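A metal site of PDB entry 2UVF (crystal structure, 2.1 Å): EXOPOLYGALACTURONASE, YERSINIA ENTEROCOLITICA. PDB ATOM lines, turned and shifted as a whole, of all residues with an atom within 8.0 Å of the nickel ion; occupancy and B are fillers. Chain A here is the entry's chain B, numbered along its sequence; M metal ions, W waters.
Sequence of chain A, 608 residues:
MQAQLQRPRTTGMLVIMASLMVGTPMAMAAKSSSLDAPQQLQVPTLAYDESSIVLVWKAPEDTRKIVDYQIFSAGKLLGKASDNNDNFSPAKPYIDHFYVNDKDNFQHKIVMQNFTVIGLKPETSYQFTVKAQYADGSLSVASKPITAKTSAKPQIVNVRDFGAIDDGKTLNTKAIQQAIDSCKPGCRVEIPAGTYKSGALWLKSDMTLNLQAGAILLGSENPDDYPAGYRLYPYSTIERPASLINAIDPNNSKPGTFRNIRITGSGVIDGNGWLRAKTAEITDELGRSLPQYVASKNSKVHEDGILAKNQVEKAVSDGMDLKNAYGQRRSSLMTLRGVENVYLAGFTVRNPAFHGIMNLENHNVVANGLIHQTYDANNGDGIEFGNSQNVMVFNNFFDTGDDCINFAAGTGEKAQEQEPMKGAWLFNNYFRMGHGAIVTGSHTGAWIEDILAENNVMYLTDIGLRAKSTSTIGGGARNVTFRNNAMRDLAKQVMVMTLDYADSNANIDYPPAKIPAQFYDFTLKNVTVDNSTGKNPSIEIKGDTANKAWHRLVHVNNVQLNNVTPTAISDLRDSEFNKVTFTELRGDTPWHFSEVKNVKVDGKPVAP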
ATOM      1  N   ALA A 295     -32.019 -19.928 -21.050  1.00  0.00           N
ATOM      2  CA  ALA A 295     -32.801 -21.165 -21.123  1.00  0.00           C
ATOM      3  C   ALA A 295     -34.208 -20.831 -21.622  1.00  0.00           C
ATOM      4  O   ALA A 295     -34.986 -20.231 -20.895  1.00  0.00           O
ATOM      5  CB  ALA A 295     -32.852 -21.832 -19.752  1.00  0.00           C
ATOM      6  N   THR A 374     -22.167 -24.680 -22.876  1.00  0.00           N
ATOM      7  CA  THR A 374     -23.426 -24.435 -23.580  1.00  0.00           C
ATOM      8  C   THR A 374     -24.629 -24.355 -22.657  1.00  0.00           C
ATOM      9  O   THR A 374     -25.773 -24.450 -23.091  1.00  0.00           O
ATOM     10  CB  THR A 374     -23.671 -25.496 -24.676  1.00  0.00           C
ATOM     11  OG1 THR A 374     -23.967 -26.774 -24.083  1.00  0.00           O
ATOM     12  CG2 THR A 374     -22.427 -25.620 -25.594  1.00  0.00           C
ATOM     13  N   TYR A 375     -24.374 -24.166 -21.360  1.00  0.00           N
ATOM     14  CA  TYR A 375     -25.461 -24.076 -20.376  1.00  0.00           C
ATOM     15  C   TYR A 375     -25.991 -22.661 -20.535  1.00  0.00           C
ATOM     16  O   TYR A 375     -25.182 -21.737 -20.551  1.00  0.00           O
ATOM     17  CB  TYR A 375     -24.883 -24.255 -18.978  1.00  0.00           C
ATOM     18  CG  TYR A 375     -25.895 -24.055 -17.915  1.00  0.00           C
ATOM     19  CD1 TYR A 375     -26.684 -25.119 -17.513  1.00  0.00           C
ATOM     20  CD2 TYR A 375     -26.126 -22.786 -17.336  1.00  0.00           C
ATOM     21  CE1 TYR A 375     -27.651 -24.976 -16.574  1.00  0.00           C
ATOM     22  CE2 TYR A 375     -27.114 -22.627 -16.376  1.00  0.00           C
ATOM     23  CZ  TYR A 375     -27.854 -23.747 -15.985  1.00  0.00           C
ATOM     24  OH  TYR A 375     -28.828 -23.676 -15.057  1.00  0.00           O
ATOM     25  N   ASP A 376     -27.324 -22.465 -20.669  1.00  0.00           N
ATOM     26  CA  ASP A 376     -28.345 -23.508 -20.624  1.00  0.00           C
ATOM     27  C   ASP A 376     -29.179 -23.449 -21.900  1.00  0.00           C
ATOM     28  O   ASP A 376     -30.424 -23.323 -21.868  1.00  0.00           O
ATOM     29  CB  ASP A 376     -29.229 -23.280 -19.385  1.00  0.00           C
ATOM     30  CG  ASP A 376     -30.049 -24.478 -19.014  1.00  0.00           C
ATOM     31  OD1 ASP A 376     -30.888 -24.359 -18.090  1.00  0.00           O
ATOM     32  OD2 ASP A 376     -29.848 -25.577 -19.620  1.00  0.00           O
ATOM     33  N   ALA A 377     -28.484 -23.561 -23.037  1.00  0.00           N
ATOM     34  CA  ALA A 377     -29.077 -23.705 -24.362  1.00  0.00           C
ATOM     35  C   ALA A 377     -29.982 -24.948 -24.479  1.00  0.00           C
ATOM     36  O   ALA A 377     -29.502 -26.080 -24.302  1.00  0.00           O
ATOM     37  CB  ALA A 377     -27.946 -23.743 -25.439  1.00  0.00           C
ATOM     38  N   ASN A 378     -31.277 -24.725 -24.792  1.00  0.00           N
ATOM     39  CA  ASN A 378     -32.282 -25.775 -24.782  1.00  0.00           C
ATOM     40  C   ASN A 378     -31.976 -26.814 -25.879  1.00  0.00           C
ATOM     41  O   ASN A 378     -31.794 -26.437 -27.039  1.00  0.00           O
ATOM     42  CB  ASN A 378     -33.671 -25.153 -24.954  1.00  0.00           C
ATOM     43  CG  ASN A 378     -34.825 -26.111 -24.663  1.00  0.00           C
ATOM     44  OD1 ASN A 378     -34.747 -27.013 -23.821  1.00  0.00           O
ATOM     45  ND2 ASN A 378     -35.889 -25.899 -25.338  1.00  0.00           N
ATOM     46  N   ASN A 379     -31.885 -28.084 -25.458  1.00  0.00           N
ATOM     47  CA  ASN A 379     -31.474 -29.222 -26.307  1.00  0.00           C
ATOM     48  C   ASN A 379     -30.000 -29.206 -26.645  1.00  0.00           C
ATOM     49  O   ASN A 379     -29.517 -29.954 -27.498  1.00  0.00           O
ATOM     50  CB  ASN A 379     -32.370 -29.355 -27.549  1.00  0.00           C
ATOM     51  CG  ASN A 379     -33.835 -29.368 -27.184  1.00  0.00           C
ATOM     52  OD1 ASN A 379     -34.574 -28.429 -27.495  1.00  0.00           O
ATOM     53  ND2 ASN A 379     -34.245 -30.390 -26.406  1.00  0.00           N
ATOM     54  N   GLY A 380     -29.269 -28.372 -25.917  1.00  0.00           N
ATOM     55  CA  GLY A 380     -27.846 -28.214 -26.163  1.00  0.00           C
ATOM     56  C   GLY A 380     -27.068 -29.292 -25.458  1.00  0.00           C
ATOM     57  O   GLY A 380     -26.305 -28.990 -24.548  1.00  0.00           O
ATOM     58  N   ASP A 381     -27.264 -30.557 -25.874  1.00  0.00           N
ATOM     59  CA  ASP A 381     -26.479 -31.660 -25.306  1.00  0.00           C
ATOM     60  C   ASP A 381     -25.044 -31.595 -25.796  1.00  0.00           C
ATOM     61  O   ASP A 381     -24.792 -31.032 -26.841  1.00  0.00           O
ATOM     62  CB  ASP A 381     -27.087 -33.063 -25.546  1.00  0.00           C
ATOM     63  CG  ASP A 381     -27.733 -33.233 -26.878  1.00  0.00           C
ATOM     64  OD1 ASP A 381     -27.355 -32.513 -27.831  1.00  0.00           O
ATOM     65  OD2 ASP A 381     -28.635 -34.116 -26.969  1.00  0.00           O
ATOM     66  N   THR A 400     -23.276 -28.226 -19.881  1.00  0.00           N
ATOM     67  CA  THR A 400     -24.141 -28.332 -21.070  1.00  0.00           C
ATOM     68  C   THR A 400     -25.568 -27.859 -20.824  1.00  0.00           C
ATOM     69  O   THR A 400     -26.085 -27.907 -19.696  1.00  0.00           O
ATOM     70  CB  THR A 400     -24.057 -29.757 -21.739  1.00  0.00           C
ATOM     71  OG1 THR A 400     -24.291 -30.773 -20.770  1.00  0.00           O
ATOM     72  CG2 THR A 400     -22.674 -30.022 -22.339  1.00  0.00           C
ATOM     73  N   GLY A 401     -26.236 -27.425 -21.903  1.00  0.00           N
ATOM     74  CA  GLY A 401     -27.649 -27.085 -21.836  1.00  0.00           C
ATOM     75  C   GLY A 401     -28.579 -28.268 -21.607  1.00  0.00           C
ATOM     76  O   GLY A 401     -29.691 -28.093 -21.099  1.00  0.00           O
ATOM     77  N   ASP A 402     -28.143 -29.466 -21.962  1.00  0.00           N
ATOM     78  CA  ASP A 402     -28.995 -30.640 -21.879  1.00  0.00           C
ATOM     79  C   ASP A 402     -28.098 -31.792 -21.485  1.00  0.00           C
ATOM     80  O   ASP A 402     -27.184 -31.615 -20.691  1.00  0.00           O
ATOM     81  CB  ASP A 402     -29.748 -30.853 -23.218  1.00  0.00           C
ATOM     82  CG  ASP A 402     -31.004 -31.704 -23.063  1.00  0.00           C
ATOM     83  OD1 ASP A 402     -30.869 -32.906 -22.759  1.00  0.00           O
ATOM     84  OD2 ASP A 402     -32.124 -31.185 -23.224  1.00  0.00           O
ATOM     85  N   ASP A 403     -28.300 -32.981 -22.054  1.00  0.00           N
ATOM     86  CA  ASP A 403     -27.526 -34.152 -21.655  1.00  0.00           C
ATOM     87  C   ASP A 403     -26.051 -33.948 -21.966  1.00  0.00           C
ATOM     88  O   ASP A 403     -25.718 -33.434 -23.019  1.00  0.00           O
ATOM     89  CB  ASP A 403     -28.025 -35.391 -22.371  1.00  0.00           C
ATOM     90  CG  ASP A 403     -29.425 -35.789 -21.963  1.00  0.00           C
ATOM     91  OD1 ASP A 403     -29.777 -35.675 -20.760  1.00  0.00           O
ATOM     92  OD2 ASP A 403     -30.157 -36.243 -22.850  1.00  0.00           O
ATOM     93  N   MET A 433     -22.471 -28.980 -15.170  1.00  0.00           N
ATOM     94  CA  MET A 433     -23.930 -28.854 -15.247  1.00  0.00           C
ATOM     95  C   MET A 433     -24.487 -29.440 -16.518  1.00  0.00           C
ATOM     96  O   MET A 433     -24.001 -29.116 -17.596  1.00  0.00           O
ATOM     97  CB  MET A 433     -24.371 -27.388 -15.118  1.00  0.00           C
ATOM     98  CG  MET A 433     -24.357 -26.847 -13.671  1.00  0.00           C
ATOM     99  SD  MET A 433     -25.271 -25.315 -13.515  1.00  0.00           S
ATOM    100  CE  MET A 433     -26.916 -25.993 -13.205  1.00  0.00           C
ATOM    101  N   GLY A 434     -25.535 -30.265 -16.408  1.00  0.00           N
ATOM    102  CA  GLY A 434     -26.127 -30.923 -17.580  1.00  0.00           C
ATOM    103  C   GLY A 434     -27.210 -31.881 -17.133  1.00  0.00           C
ATOM    104  O   GLY A 434     -27.374 -32.111 -15.940  1.00  0.00           O
ATOM    105  N   HIS A 435     -27.957 -32.442 -18.061  1.00  0.00           N
ATOM    106  CA  HIS A 435     -29.149 -33.206 -17.660  1.00  0.00           C
ATOM    107  C   HIS A 435     -28.905 -34.650 -17.166  1.00  0.00           C
ATOM    108  O   HIS A 435     -29.793 -35.281 -16.610  1.00  0.00           O
ATOM    109  CB  HIS A 435     -30.173 -33.171 -18.761  1.00  0.00           C
ATOM    110  CG  HIS A 435     -30.783 -31.832 -18.985  1.00  0.00           C
ATOM    111  ND1 HIS A 435     -31.938 -31.669 -19.702  1.00  0.00           N
ATOM    112  CD2 HIS A 435     -30.411 -30.603 -18.571  1.00  0.00           C
ATOM    113  CE1 HIS A 435     -32.250 -30.375 -19.737  1.00  0.00           C
ATOM    114  NE2 HIS A 435     -31.330 -29.710 -19.066  1.00  0.00           N
ATOM    115  N   ASP A 462     -27.262 -32.830 -13.052  1.00  0.00           N
ATOM    116  CA  ASP A 462     -28.559 -33.368 -12.634  1.00  0.00           C
ATOM    117  C   ASP A 462     -28.487 -34.813 -12.174  1.00  0.00           C
ATOM    118  O   ASP A 462     -28.828 -35.147 -11.028  1.00  0.00           O
ATOM    119  CB  ASP A 462     -29.579 -33.243 -13.741  1.00  0.00           C
ATOM    120  CG  ASP A 462     -30.043 -31.832 -13.948  1.00  0.00           C
ATOM    121  OD1 ASP A 462     -29.419 -30.886 -13.393  1.00  0.00           O
ATOM    122  OD2 ASP A 462     -31.033 -31.672 -14.713  1.00  0.00           O
HETATM  123 NI    NI M   1     -30.435 -27.571 -19.198  1.00  0.00          NI
HETATM  124  O   HOH W   1     -32.158 -27.160 -20.182  1.00  0.00           O
HETATM  125  O   HOH W   2     -28.396 -27.833 -18.370  1.00  0.00           O
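N of Gly 401 sits at hydrogen-bond distance from OG1 of Thr 374, 3.2 Å away.
The backbone carbonyl oxygen (O) of Gly 380 lies within hydrogen-bond range of the backbone NH (N) of Gly 401, 3.1 Å away.
The backbone NH (N) of His 435 is in hydrogen-bond range of the backbone carbonyl oxygen (O) of Asp 402 (2.9 Å).
Within 4 Å of the nickel ion: Asp 376, Gly 401 and His 435.
The nickel ion is bound by water W1 (2.0 Å), the backbone carbonyl oxygen (O) of Gly 401 (2.1 Å), the side-chain carboxylate (OD2) of Asp 376 (2.1 Å), water W2 (2.2 Å) and a ring nitrogen (NE2) of His 435 (2.3 Å).
The nickel ion has five donor atoms within binding distance.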
